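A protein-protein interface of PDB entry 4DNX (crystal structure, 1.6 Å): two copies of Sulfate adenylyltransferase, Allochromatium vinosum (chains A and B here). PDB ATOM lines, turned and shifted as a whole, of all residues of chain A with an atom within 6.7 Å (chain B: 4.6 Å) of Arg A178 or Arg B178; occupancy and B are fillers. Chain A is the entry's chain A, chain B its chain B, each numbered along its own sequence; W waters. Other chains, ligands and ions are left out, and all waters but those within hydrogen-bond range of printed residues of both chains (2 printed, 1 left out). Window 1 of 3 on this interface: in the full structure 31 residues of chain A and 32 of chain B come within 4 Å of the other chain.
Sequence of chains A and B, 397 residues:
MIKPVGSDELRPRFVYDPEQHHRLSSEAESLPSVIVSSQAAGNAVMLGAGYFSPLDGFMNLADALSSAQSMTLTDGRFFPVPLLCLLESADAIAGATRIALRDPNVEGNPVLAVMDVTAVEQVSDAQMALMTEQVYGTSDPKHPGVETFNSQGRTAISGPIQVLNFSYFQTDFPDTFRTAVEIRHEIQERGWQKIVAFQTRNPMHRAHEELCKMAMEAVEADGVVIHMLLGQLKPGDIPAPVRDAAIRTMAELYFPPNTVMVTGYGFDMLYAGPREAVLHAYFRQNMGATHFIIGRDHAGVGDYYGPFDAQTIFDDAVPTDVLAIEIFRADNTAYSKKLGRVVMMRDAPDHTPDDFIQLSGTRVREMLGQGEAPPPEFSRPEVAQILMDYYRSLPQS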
ATOM      1  N   ALA A  49      14.188  -1.676 -19.537  1.00  0.00           N
ATOM      2  CA  ALA A  49      13.029  -2.611 -19.443  1.00  0.00           C
ATOM      3  C   ALA A  49      12.420  -2.603 -18.046  1.00  0.00           C
ATOM      4  O   ALA A  49      11.438  -3.322 -17.795  1.00  0.00           O
ATOM      5  CB  ALA A  49      13.505  -4.019 -19.805  1.00  0.00           C
ATOM      6  N   TYR A  51      13.686  -3.623 -15.187  1.00  0.00           N
ATOM      7  CA  TYR A  51      14.190  -4.629 -14.260  1.00  0.00           C
ATOM      8  C   TYR A  51      15.076  -4.022 -13.146  1.00  0.00           C
ATOM      9  O   TYR A  51      15.115  -4.543 -12.018  1.00  0.00           O
ATOM     10  CB  TYR A  51      14.975  -5.682 -15.020  1.00  0.00           C
ATOM     11  CG  TYR A  51      14.089  -6.630 -15.823  1.00  0.00           C
ATOM     12  CD1 TYR A  51      13.267  -7.563 -15.165  1.00  0.00           C
ATOM     13  CD2 TYR A  51      14.092  -6.606 -17.232  1.00  0.00           C
ATOM     14  CE1 TYR A  51      12.449  -8.442 -15.895  1.00  0.00           C
ATOM     15  CE2 TYR A  51      13.312  -7.459 -17.995  1.00  0.00           C
ATOM     16  CZ  TYR A  51      12.482  -8.399 -17.306  1.00  0.00           C
ATOM     17  OH  TYR A  51      11.723  -9.265 -18.044  1.00  0.00           O
ATOM     18  N   GLN A 170      15.338  -8.379 -28.161  1.00  0.00           N
ATOM     19  CA  GLN A 170      14.002  -8.256 -28.755  1.00  0.00           C
ATOM     20  C   GLN A 170      13.944  -8.664 -30.204  1.00  0.00           C
ATOM     21  O   GLN A 170      13.051  -9.441 -30.570  1.00  0.00           O
ATOM     22  CB  GLN A 170      13.319  -6.877 -28.546  1.00  0.00           C
ATOM     23  CG  GLN A 170      11.782  -7.013 -28.815  1.00  0.00           C
ATOM     24  CD  GLN A 170      10.954  -5.834 -28.310  1.00  0.00           C
ATOM     25  OE1 GLN A 170      11.345  -4.683 -28.508  1.00  0.00           O
ATOM     26  NE2 GLN A 170       9.770  -6.132 -27.693  1.00  0.00           N
ATOM     27  N   PHE A 173      14.280 -12.537 -30.451  1.00  0.00           N
ATOM     28  CA  PHE A 173      13.325 -13.342 -29.661  1.00  0.00           C
ATOM     29  C   PHE A 173      11.994 -12.544 -29.494  1.00  0.00           C
ATOM     30  O   PHE A 173      11.596 -12.232 -28.355  1.00  0.00           O
ATOM     31  CB  PHE A 173      13.936 -13.711 -28.293  1.00  0.00           C
ATOM     32  CG  PHE A 173      15.339 -14.311 -28.386  1.00  0.00           C
ATOM     33  CD1 PHE A 173      15.536 -15.665 -28.653  1.00  0.00           C
ATOM     34  CD2 PHE A 173      16.450 -13.507 -28.216  1.00  0.00           C
ATOM     35  CE1 PHE A 173      16.834 -16.179 -28.728  1.00  0.00           C
ATOM     36  CE2 PHE A 173      17.739 -14.029 -28.295  1.00  0.00           C
ATOM     37  CZ  PHE A 173      17.935 -15.342 -28.533  1.00  0.00           C
ATOM     38  N   PRO A 174      11.359 -12.181 -30.609  1.00  0.00           N
ATOM     39  CA  PRO A 174      10.240 -11.199 -30.524  1.00  0.00           C
ATOM     40  C   PRO A 174       9.050 -11.678 -29.722  1.00  0.00           C
ATOM     41  O   PRO A 174       8.325 -10.801 -29.161  1.00  0.00           O
ATOM     42  CB  PRO A 174       9.849 -10.936 -31.984  1.00  0.00           C
ATOM     43  CG  PRO A 174      10.255 -12.265 -32.737  1.00  0.00           C
ATOM     44  CD  PRO A 174      11.578 -12.612 -32.015  1.00  0.00           C
ATOM     45  N   ASP A 175       8.813 -12.985 -29.659  1.00  0.00           N
ATOM     46  CA  ASP A 175       7.643 -13.510 -28.912  1.00  0.00           C
ATOM     47  C   ASP A 175       7.882 -13.721 -27.433  1.00  0.00           C
ATOM     48  O   ASP A 175       6.925 -13.813 -26.649  1.00  0.00           O
ATOM     49  CB  ASP A 175       7.096 -14.818 -29.535  1.00  0.00           C
ATOM     50  CG  ASP A 175       6.525 -14.610 -30.946  1.00  0.00           C
ATOM     51  OD1 ASP A 175       6.167 -13.443 -31.314  1.00  0.00           O
ATOM     52  OD2 ASP A 175       6.397 -15.598 -31.696  1.00  0.00           O
ATOM     53  N   THR A 176       9.143 -13.807 -27.016  1.00  0.00           N
ATOM     54  CA  THR A 176       9.439 -14.156 -25.651  1.00  0.00           C
ATOM     55  C   THR A 176      10.042 -13.015 -24.828  1.00  0.00           C
ATOM     56  O   THR A 176       9.765 -12.914 -23.642  1.00  0.00           O
ATOM     57  CB  THR A 176      10.351 -15.411 -25.540  1.00  0.00           C
ATOM     58  OG1 THR A 176      11.494 -15.226 -26.366  1.00  0.00           O
ATOM     59  CG2 THR A 176       9.588 -16.644 -26.045  1.00  0.00           C
ATOM     60  N   PHE A 177      10.854 -12.147 -25.454  1.00  0.00           N
ATOM     61  CA  PHE A 177      11.424 -11.040 -24.720  1.00  0.00           C
ATOM     62  C   PHE A 177      10.312 -10.178 -24.151  1.00  0.00           C
ATOM     63  O   PHE A 177       9.393  -9.817 -24.895  1.00  0.00           O
ATOM     64  CB  PHE A 177      12.348 -10.152 -25.574  1.00  0.00           C
ATOM     65  CG  PHE A 177      12.873  -8.978 -24.820  1.00  0.00           C
ATOM     66  CD1 PHE A 177      13.998  -9.101 -23.993  1.00  0.00           C
ATOM     67  CD2 PHE A 177      12.172  -7.735 -24.852  1.00  0.00           C
ATOM     68  CE1 PHE A 177      14.464  -7.999 -23.253  1.00  0.00           C
ATOM     69  CE2 PHE A 177      12.602  -6.645 -24.057  1.00  0.00           C
ATOM     70  CZ  PHE A 177      13.770  -6.776 -23.295  1.00  0.00           C
ATOM     71  N   ARG A 178      10.423  -9.881 -22.837  1.00  0.00           N
ATOM     72  CA  ARG A 178       9.427  -9.029 -22.133  1.00  0.00           C
ATOM     73  C   ARG A 178      10.129  -8.074 -21.197  1.00  0.00           C
ATOM     74  O   ARG A 178      11.134  -8.417 -20.597  1.00  0.00           O
ATOM     75  CB  ARG A 178       8.521  -9.889 -21.225  1.00  0.00           C
ATOM     76  CG  ARG A 178       7.604 -10.710 -22.007  1.00  0.00           C
ATOM     77  CD  ARG A 178       6.404  -9.915 -22.523  1.00  0.00           C
ATOM     78  NE  ARG A 178       5.474 -10.887 -23.059  1.00  0.00           N
ATOM     79  CZ  ARG A 178       5.618 -11.521 -24.224  1.00  0.00           C
ATOM     80  NH1 ARG A 178       6.641 -11.250 -25.045  1.00  0.00           N
ATOM     81  NH2 ARG A 178       4.712 -12.426 -24.584  1.00  0.00           N
ATOM     82  N   THR A 179       9.566  -6.884 -21.076  1.00  0.00           N
ATOM     83  CA  THR A 179      10.009  -5.948 -20.061  1.00  0.00           C
ATOM     84  C   THR A 179       9.410  -6.332 -18.722  1.00  0.00           C
ATOM     85  O   THR A 179       8.391  -7.053 -18.666  1.00  0.00           O
ATOM     86  CB  THR A 179       9.558  -4.501 -20.393  1.00  0.00           C
ATOM     87  OG1 THR A 179       8.117  -4.439 -20.455  1.00  0.00           O
ATOM     88  CG2 THR A 179      10.176  -4.064 -21.742  1.00  0.00           C
ATOM     89  N   ALA A 180      10.011  -5.834 -17.637  1.00  0.00           N
ATOM     90  CA  ALA A 180       9.399  -6.018 -16.290  1.00  0.00           C
ATOM     91  C   ALA A 180       8.027  -5.322 -16.270  1.00  0.00           C
ATOM     92  O   ALA A 180       7.100  -5.790 -15.594  1.00  0.00           O
ATOM     93  CB  ALA A 180      10.279  -5.378 -15.216  1.00  0.00           C
ATOM     94  N   VAL A 181       7.910  -4.200 -16.986  1.00  0.00           N
ATOM     95  CA  VAL A 181       6.670  -3.443 -17.072  1.00  0.00           C
ATOM     96  C   VAL A 181       5.538  -4.348 -17.629  1.00  0.00           C
ATOM     97  O   VAL A 181       4.432  -4.419 -17.045  1.00  0.00           O
ATOM     98  CB  VAL A 181       6.855  -2.169 -17.952  1.00  0.00           C
ATOM     99  CG1 VAL A 181       5.502  -1.511 -18.258  1.00  0.00           C
ATOM    100  CG2 VAL A 181       7.874  -1.185 -17.274  1.00  0.00           C
ATOM    101  N   GLU A 182       5.832  -5.058 -18.712  1.00  0.00           N
ATOM    102  CA  GLU A 182       4.770  -5.858 -19.366  1.00  0.00           C
ATOM    103  C   GLU A 182       4.474  -7.133 -18.566  1.00  0.00           C
ATOM    104  O   GLU A 182       3.296  -7.552 -18.524  1.00  0.00           O
ATOM    105  CB  GLU A 182       5.176  -6.208 -20.794  1.00  0.00           C
ATOM    106  CG  GLU A 182       4.085  -6.979 -21.626  1.00  0.00           C
ATOM    107  CD  GLU A 182       2.681  -6.306 -21.691  1.00  0.00           C
ATOM    108  OE1 GLU A 182       2.523  -5.083 -21.433  1.00  0.00           O
ATOM    109  OE2 GLU A 182       1.711  -7.025 -22.064  1.00  0.00           O
ATOM    110  N   ILE A 183       5.495  -7.720 -17.945  1.00  0.00           N
ATOM    111  CA  ILE A 183       5.235  -8.920 -17.080  1.00  0.00           C
ATOM    112  C   ILE A 183       4.307  -8.506 -15.925  1.00  0.00           C
ATOM    113  O   ILE A 183       3.293  -9.211 -15.638  1.00  0.00           O
ATOM    114  CB  ILE A 183       6.536  -9.506 -16.588  1.00  0.00           C
ATOM    115  CG1 ILE A 183       7.246 -10.173 -17.768  1.00  0.00           C
ATOM    116  CG2 ILE A 183       6.298 -10.504 -15.500  1.00  0.00           C
ATOM    117  CD1 ILE A 183       8.682 -10.714 -17.454  1.00  0.00           C
ATOM    118  N   GLU A 186       0.697  -8.106 -17.252  1.00  0.00           N
ATOM    119  CA  GLU A 186       0.115  -9.428 -17.523  1.00  0.00           C
ATOM    120  C   GLU A 186      -0.237 -10.215 -16.255  1.00  0.00           C
ATOM    121  O   GLU A 186      -1.301 -10.843 -16.208  1.00  0.00           O
ATOM    122  CB  GLU A 186       1.014 -10.250 -18.432  1.00  0.00           C
ATOM    123  CG  GLU A 186       0.526 -11.675 -18.678  1.00  0.00           C
ATOM    124  CD  GLU A 186       1.058 -12.283 -19.971  1.00  0.00           C
ATOM    125  OE1 GLU A 186       0.539 -13.361 -20.334  1.00  0.00           O
ATOM    126  OE2 GLU A 186       1.980 -11.690 -20.621  1.00  0.00           O
ATOM    127  N   HIS A 227      11.118 -17.592 -16.628  1.00  0.00           N
ATOM    128  CA  HIS A 227      11.812 -16.354 -17.052  1.00  0.00           C
ATOM    129  C   HIS A 227      13.104 -16.841 -17.711  1.00  0.00           C
ATOM    130  O   HIS A 227      14.072 -17.172 -17.023  1.00  0.00           O
ATOM    131  CB  HIS A 227      12.047 -15.500 -15.804  1.00  0.00           C
ATOM    132  CG  HIS A 227      12.218 -14.028 -16.094  1.00  0.00           C
ATOM    133  ND1 HIS A 227      13.057 -13.226 -15.349  1.00  0.00           N
ATOM    134  CD2 HIS A 227      11.694 -13.237 -17.052  1.00  0.00           C
ATOM    135  CE1 HIS A 227      13.012 -11.983 -15.808  1.00  0.00           C
ATOM    136  NE2 HIS A 227      12.199 -11.960 -16.854  1.00  0.00           N
ATOM    137  N   LEU A 230      17.728 -15.059 -22.270  1.00  0.00           N
ATOM    138  CA  LEU A 230      17.957 -14.960 -23.699  1.00  0.00           C
ATOM    139  C   LEU A 230      19.389 -14.489 -23.965  1.00  0.00           C
ATOM    140  O   LEU A 230      19.904 -13.631 -23.251  1.00  0.00           O
ATOM    141  CB  LEU A 230      16.998 -13.914 -24.305  1.00  0.00           C
ATOM    142  CG  LEU A 230      15.548 -14.259 -23.957  1.00  0.00           C
ATOM    143  CD1 LEU A 230      14.656 -13.082 -24.384  1.00  0.00           C
ATOM    144  CD2 LEU A 230      15.079 -15.537 -24.610  1.00  0.00           C
ATOM    145  N   ARG A 248       6.795 -24.577 -24.096  1.00  0.00           N
ATOM    146  CA  ARG A 248       5.366 -24.247 -24.327  1.00  0.00           C
ATOM    147  C   ARG A 248       4.518 -25.495 -24.352  1.00  0.00           C
ATOM    148  O   ARG A 248       3.368 -25.481 -23.878  1.00  0.00           O
ATOM    149  CB  ARG A 248       5.167 -23.471 -25.613  1.00  0.00           C
ATOM    150  CG  ARG A 248       5.667 -22.041 -25.488  1.00  0.00           C
ATOM    151  CD  ARG A 248       5.367 -21.337 -26.803  1.00  0.00           C
ATOM    152  NE  ARG A 248       6.119 -20.086 -27.001  1.00  0.00           N
ATOM    153  CZ  ARG A 248       5.839 -18.925 -26.407  1.00  0.00           C
ATOM    154  NH1 ARG A 248       4.852 -18.826 -25.517  1.00  0.00           N
ATOM    155  NH2 ARG A 248       6.557 -17.845 -26.710  1.00  0.00           N
ATOM    156  N   MET A 261       3.265 -18.437 -17.363  1.00  0.00           N
ATOM    157  CA  MET A 261       3.659 -17.396 -18.286  1.00  0.00           C
ATOM    158  C   MET A 261       5.075 -17.681 -18.758  1.00  0.00           C
ATOM    159  O   MET A 261       5.966 -17.743 -17.938  1.00  0.00           O
ATOM    160  CB  MET A 261       3.676 -16.051 -17.562  1.00  0.00           C
ATOM    161  CG  MET A 261       2.386 -15.345 -17.538  1.00  0.00           C
ATOM    162  SD  MET A 261       2.539 -13.862 -16.494  1.00  0.00           S
ATOM    163  CE  MET A 261       3.861 -13.001 -17.344  1.00  0.00           C
ATOM    164  N   VAL A 262       5.259 -17.856 -20.068  1.00  0.00           N
ATOM    165  CA  VAL A 262       6.594 -18.115 -20.664  1.00  0.00           C
ATOM    166  C   VAL A 262       7.168 -16.803 -21.213  1.00  0.00           C
ATOM    167  O   VAL A 262       6.545 -16.126 -22.074  1.00  0.00           O
ATOM    168  CB  VAL A 262       6.531 -19.197 -21.754  1.00  0.00           C
ATOM    169  CG1 VAL A 262       7.919 -19.461 -22.364  1.00  0.00           C
ATOM    170  CG2 VAL A 262       5.998 -20.534 -21.152  1.00  0.00           C
ATOM    171  N   THR A 263       8.333 -16.431 -20.692  1.00  0.00           N
ATOM    172  CA  THR A 263       8.850 -15.065 -20.938  1.00  0.00           C
ATOM    173  C   THR A 263      10.347 -15.151 -20.955  1.00  0.00           C
ATOM    174  O   THR A 263      10.936 -16.198 -20.638  1.00  0.00           O
ATOM    175  CB  THR A 263       8.511 -14.092 -19.781  1.00  0.00           C
ATOM    176  OG1 THR A 263       9.240 -14.462 -18.607  1.00  0.00           O
ATOM    177  CG2 THR A 263       6.985 -14.044 -19.494  1.00  0.00           C
ATOM    178  N   GLY A 264      10.972 -14.027 -21.258  1.00  0.00           N
ATOM    179  CA  GLY A 264      12.440 -13.979 -21.285  1.00  0.00           C
ATOM    180  C   GLY A 264      13.005 -12.591 -21.086  1.00  0.00           C
ATOM    181  O   GLY A 264      12.297 -11.565 -21.245  1.00  0.00           O
ATOM    182  N   TYR A 265      14.298 -12.542 -20.757  1.00  0.00           N
ATOM    183  CA  TYR A 265      14.941 -11.260 -20.560  1.00  0.00           C
ATOM    184  C   TYR A 265      16.373 -11.363 -21.066  1.00  0.00           C
ATOM    185  O   TYR A 265      16.871 -12.450 -21.319  1.00  0.00           O
ATOM    186  CB  TYR A 265      14.922 -10.878 -19.067  1.00  0.00           C
ATOM    187  CG  TYR A 265      15.826 -11.732 -18.202  1.00  0.00           C
ATOM    188  CD1 TYR A 265      15.505 -13.049 -17.912  1.00  0.00           C
ATOM    189  CD2 TYR A 265      17.072 -11.230 -17.773  1.00  0.00           C
ATOM    190  CE1 TYR A 265      16.334 -13.817 -17.154  1.00  0.00           C
ATOM    191  CE2 TYR A 265      17.936 -12.017 -17.010  1.00  0.00           C
ATOM    192  CZ  TYR A 265      17.554 -13.309 -16.733  1.00  0.00           C
ATOM    193  OH  TYR A 265      18.376 -14.078 -15.949  1.00  0.00           O
ATOM    194  N   GLY A 266      17.013 -10.203 -21.199  1.00  0.00           N
ATOM    195  CA  GLY A 266      18.405 -10.174 -21.711  1.00  0.00           C
ATOM    196  C   GLY A 266      19.361  -9.455 -20.763  1.00  0.00           C
ATOM    197  O   GLY A 266      19.154  -8.281 -20.450  1.00  0.00           O
ATOM    198  N   TYR B  51       0.154 -13.154 -39.396  1.00  0.00           N
ATOM    199  CA  TYR B  51      -1.223 -12.693 -39.591  1.00  0.00           C
ATOM    200  C   TYR B  51      -1.773 -13.082 -40.989  1.00  0.00           C
ATOM    201  O   TYR B  51      -2.976 -13.335 -41.147  1.00  0.00           O
ATOM    202  CB  TYR B  51      -1.272 -11.183 -39.439  1.00  0.00           C
ATOM    203  CG  TYR B  51      -1.204 -10.719 -37.983  1.00  0.00           C
ATOM    204  CD1 TYR B  51      -2.272 -10.974 -37.122  1.00  0.00           C
ATOM    205  CD2 TYR B  51      -0.051 -10.026 -37.471  1.00  0.00           C
ATOM    206  CE1 TYR B  51      -2.232 -10.564 -35.774  1.00  0.00           C
ATOM    207  CE2 TYR B  51       0.005  -9.602 -36.125  1.00  0.00           C
ATOM    208  CZ  TYR B  51      -1.092  -9.850 -35.309  1.00  0.00           C
ATOM    209  OH  TYR B  51      -1.065  -9.429 -33.990  1.00  0.00           O
ATOM    210  N   PRO B 174       7.035  -1.666 -27.773  1.00  0.00           N
ATOM    211  CA  PRO B 174       7.589  -2.997 -27.349  1.00  0.00           C
ATOM    212  C   PRO B 174       6.686  -3.815 -26.414  1.00  0.00           C
ATOM    213  O   PRO B 174       6.779  -5.062 -26.433  1.00  0.00           O
ATOM    214  CB  PRO B 174       8.907  -2.619 -26.658  1.00  0.00           C
ATOM    215  CG  PRO B 174       8.578  -1.240 -26.045  1.00  0.00           C
ATOM    216  CD  PRO B 174       7.900  -0.580 -27.297  1.00  0.00           C
ATOM    217  N   ASP B 175       5.824  -3.163 -25.635  1.00  0.00           N
ATOM    218  CA  ASP B 175       4.958  -3.921 -24.731  1.00  0.00           C
ATOM    219  C   ASP B 175       3.626  -4.295 -25.339  1.00  0.00           C
ATOM    220  O   ASP B 175       2.900  -5.125 -24.741  1.00  0.00           O
ATOM    221  CB  ASP B 175       4.703  -3.134 -23.467  1.00  0.00           C
ATOM    222  CG  ASP B 175       5.974  -2.963 -22.599  1.00  0.00           C
ATOM    223  OD1 ASP B 175       7.013  -3.706 -22.774  1.00  0.00           O
ATOM    224  OD2 ASP B 175       5.945  -2.095 -21.679  1.00  0.00           O
ATOM    225  N   THR B 176       3.289  -3.703 -26.491  1.00  0.00           N
ATOM    226  CA  THR B 176       1.958  -3.980 -27.046  1.00  0.00           C
ATOM    227  C   THR B 176       1.973  -4.683 -28.397  1.00  0.00           C
ATOM    228  O   THR B 176       1.079  -5.482 -28.659  1.00  0.00           O
ATOM    229  CB  THR B 176       1.053  -2.731 -27.125  1.00  0.00           C
ATOM    230  OG1 THR B 176       1.730  -1.728 -27.876  1.00  0.00           O
ATOM    231  CG2 THR B 176       0.743  -2.198 -25.756  1.00  0.00           C
ATOM    232  N   PHE B 177       2.958  -4.436 -29.260  1.00  0.00           N
ATOM    233  CA  PHE B 177       3.012  -5.134 -30.548  1.00  0.00           C
ATOM    234  C   PHE B 177       3.100  -6.625 -30.294  1.00  0.00           C
ATOM    235  O   PHE B 177       3.900  -7.065 -29.468  1.00  0.00           O
ATOM    236  CB  PHE B 177       4.273  -4.737 -31.345  1.00  0.00           C
ATOM    237  CG  PHE B 177       4.425  -5.526 -32.636  1.00  0.00           C
ATOM    238  CD1 PHE B 177       3.726  -5.175 -33.765  1.00  0.00           C
ATOM    239  CD2 PHE B 177       5.225  -6.679 -32.680  1.00  0.00           C
ATOM    240  CE1 PHE B 177       3.812  -5.907 -34.969  1.00  0.00           C
ATOM    241  CE2 PHE B 177       5.305  -7.465 -33.892  1.00  0.00           C
ATOM    242  CZ  PHE B 177       4.605  -7.068 -35.021  1.00  0.00           C
ATOM    243  N   ARG B 178       2.296  -7.408 -31.002  1.00  0.00           N
ATOM    244  CA  ARG B 178       2.351  -8.863 -30.798  1.00  0.00           C
ATOM    245  C   ARG B 178       2.197  -9.526 -32.140  1.00  0.00           C
ATOM    246  O   ARG B 178       1.436  -9.063 -32.969  1.00  0.00           O
ATOM    247  CB  ARG B 178       1.109  -9.343 -29.997  1.00  0.00           C
ATOM    248  CG  ARG B 178       1.144  -9.040 -28.524  1.00  0.00           C
ATOM    249  CD  ARG B 178       2.038 -10.051 -27.827  1.00  0.00           C
ATOM    250  NE  ARG B 178       2.119  -9.861 -26.387  1.00  0.00           N
ATOM    251  CZ  ARG B 178       2.804  -8.888 -25.778  1.00  0.00           C
ATOM    252  NH1 ARG B 178       3.448  -7.947 -26.479  1.00  0.00           N
ATOM    253  NH2 ARG B 178       2.819  -8.836 -24.448  1.00  0.00           N
ATOM    254  N   THR B 179       2.856 -10.666 -32.323  1.00  0.00           N
ATOM    255  CA  THR B 179       2.610 -11.477 -33.536  1.00  0.00           C
ATOM    256  C   THR B 179       1.330 -12.317 -33.370  1.00  0.00           C
ATOM    257  O   THR B 179       0.858 -12.527 -32.224  1.00  0.00           O
ATOM    258  CB  THR B 179       3.773 -12.465 -33.810  1.00  0.00           C
ATOM    259  OG1 THR B 179       3.955 -13.322 -32.672  1.00  0.00           O
ATOM    260  CG2 THR B 179       5.069 -11.669 -34.015  1.00  0.00           C
ATOM    261  N   ALA B 180       0.801 -12.826 -34.474  1.00  0.00           N
ATOM    262  CA  ALA B 180      -0.374 -13.763 -34.419  1.00  0.00           C
ATOM    263  C   ALA B 180       0.058 -14.984 -33.655  1.00  0.00           C
ATOM    264  O   ALA B 180      -0.719 -15.557 -32.871  1.00  0.00           O
ATOM    265  CB  ALA B 180      -0.859 -14.123 -35.858  1.00  0.00           C
ATOM    266  N   GLU B 182       2.256 -15.238 -31.127  1.00  0.00           N
ATOM    267  CA  GLU B 182       2.264 -15.014 -29.688  1.00  0.00           C
ATOM    268  C   GLU B 182       0.879 -14.856 -29.113  1.00  0.00           C
ATOM    269  O   GLU B 182       0.637 -15.314 -28.010  1.00  0.00           O
ATOM    270  CB  GLU B 182       3.164 -13.814 -29.287  1.00  0.00           C
ATOM    271  CG  GLU B 182       3.290 -13.564 -27.779  1.00  0.00           C
ATOM    272  CD  GLU B 182       3.793 -14.758 -26.942  1.00  0.00           C
ATOM    273  OE1 GLU B 182       4.313 -15.777 -27.463  1.00  0.00           O
ATOM    274  OE2 GLU B 182       3.729 -14.654 -25.711  1.00  0.00           O
ATOM    275  N   ILE B 183      -0.003 -14.208 -29.854  1.00  0.00           N
ATOM    276  CA  ILE B 183      -1.392 -14.050 -29.374  1.00  0.00           C
ATOM    277  C   ILE B 183      -2.022 -15.453 -29.232  1.00  0.00           C
ATOM    278  O   ILE B 183      -2.612 -15.759 -28.171  1.00  0.00           O
ATOM    279  CB  ILE B 183      -2.197 -13.192 -30.330  1.00  0.00           C
ATOM    280  CG1 ILE B 183      -1.739 -11.724 -30.166  1.00  0.00           C
ATOM    281  CG2 ILE B 183      -3.743 -13.294 -29.988  1.00  0.00           C
ATOM    282  CD1 ILE B 183      -2.338 -10.678 -31.097  1.00  0.00           C
ATOM    283  N   GLU B 186      -0.666 -17.111 -26.053  1.00  0.00           N
ATOM    284  CA  GLU B 186      -1.160 -16.504 -24.824  1.00  0.00           C
ATOM    285  C   GLU B 186      -2.616 -16.922 -24.579  1.00  0.00           C
ATOM    286  O   GLU B 186      -3.002 -17.184 -23.434  1.00  0.00           O
ATOM    287  CB  GLU B 186      -1.130 -14.962 -24.865  1.00  0.00           C
ATOM    288  CG  GLU B 186      -1.318 -14.378 -23.458  1.00  0.00           C
ATOM    289  CD  GLU B 186      -1.040 -12.881 -23.300  1.00  0.00           C
ATOM    290  OE1 GLU B 186      -1.587 -12.307 -22.319  1.00  0.00           O
ATOM    291  OE2 GLU B 186      -0.259 -12.299 -24.122  1.00  0.00           O
ATOM    292  N   THR B 263      -3.291  -5.721 -26.862  1.00  0.00           N
ATOM    293  CA  THR B 263      -2.269  -6.096 -27.862  1.00  0.00           C
ATOM    294  C   THR B 263      -2.341  -5.129 -29.022  1.00  0.00           C
ATOM    295  O   THR B 263      -3.270  -4.331 -29.131  1.00  0.00           O
ATOM    296  CB  THR B 263      -2.518  -7.518 -28.474  1.00  0.00           C
ATOM    297  OG1 THR B 263      -3.731  -7.493 -29.268  1.00  0.00           O
ATOM    298  CG2 THR B 263      -2.592  -8.600 -27.421  1.00  0.00           C
ATOM    299  N   GLY B 264      -1.383  -5.227 -29.952  1.00  0.00           N
ATOM    300  CA  GLY B 264      -1.427  -4.384 -31.145  1.00  0.00           C
ATOM    301  C   GLY B 264      -0.773  -5.077 -32.322  1.00  0.00           C
ATOM    302  O   GLY B 264      -0.071  -6.094 -32.154  1.00  0.00           O
HETATM  303  O   HOH W   1       7.603  -6.312 -23.257  1.00  0.00           O
HETATM  304  O   HOH W   2       4.999 -11.080 -30.359  1.00  0.00           O
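NE2 of Gln A170 lies within hydrogen-bond range of O of Pro B174 (3.4 Å).
The side-chain carboxylate of Asp A175 sits at hydrogen-bond distance from the side-chain hydroxyl of Thr B179 (2.6 Å).
The guanidinium group (NH2) of Arg A178 lies within salt-bridge range of the side-chain carboxylate (OE2) of Glu B182 (2.7 Å).
OD1 of Asp B175 lies within hydrogen-bond range of OG1 of Thr A179 (2.7 Å).
The side-chain carboxylate of Glu A182 is in salt-bridge range of the guanidinium group of Arg B178 (3.2 Å).
NH2 of Arg A248 lies within salt-bridge range of OE1 of Glu B182 (3.1 Å).
O of Asp A175 sits close to OE1 of Glu B182, at 3.4 Å.
The backbone carbonyl oxygen (O) of Asp B175 sits close to the side-chain carboxylate (OE1) of Glu A182 (3.3 Å).
The side-chain carboxylate (OE1) of Glu A186 lies close to the side-chain carboxylate (OE1) of Glu B186 (3.1 Å).
O of Arg A178 lies within hydrogen-bond range of OH of Tyr A51 (2.8 Å).
The side-chain hydroxyl (OG1) of Thr A179 lies within hydrogen-bond range of the backbone NH (N) of Glu A182, at 2.9 Å.
Among the printed residues, merely in contact across the chains: Val A181 with Asp B175 and Arg A178 with Arg B178.
Of the printed residues of chain B, Arg A178 touches Arg B178 and Glu B182.
Of the printed residues of chain A, Pro B174 touches Gln A170.
Printed residues of chain A within 4 Å of Glu B186: Glu A186 (3.1 Å).
The nearest printed residue of chain B that does not touch Arg A178 is Glu B186 (5.0 Å).
The nearest printed residue of chain A that does not touch Arg B178 is Glu A186 (4.8 Å).
Of the 13 printed residues of chain B, 6 touch a printed residue of chain A.
Hydrophobic or aromatic side chains of chain B that line the printed part of chain A: Pro B174.
Printed residues of chain A that touch a printed residue of chain B: Gln A170, Asp A175, Arg A178, Thr A179, Val A181, Glu A182, Glu A186 and Arg A248.
Hydrophobic or aromatic side chains of chain A that line the printed part of chain B: Val A181.
Along chain A the printed residues that touch a printed residue of chain B span positions 170 to 248.
Among the printed residues, Asp or Glu carboxylates within 4 Å of a Lys or Arg side-chain nitrogen of the other chain: Arg A178 with Glu B182, Glu A182 with Arg B178 and Arg A248 with Glu B182.
Arg B178 touches its own counterpart, Arg A178.
Arg A178 touches Glu B182, and with the chains exchanged Glu A182 touches Arg B178.
Glu B186 touches its own counterpart, Glu A186.
Water W1 lies within hydrogen-bond range of OD1 of Asp B175 and N of Thr A179.
Water W2 bridges the side-chain carboxylate of Asp A175 (2.8 Å) and the backbone NH of Thr B179 (2.9 Å).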
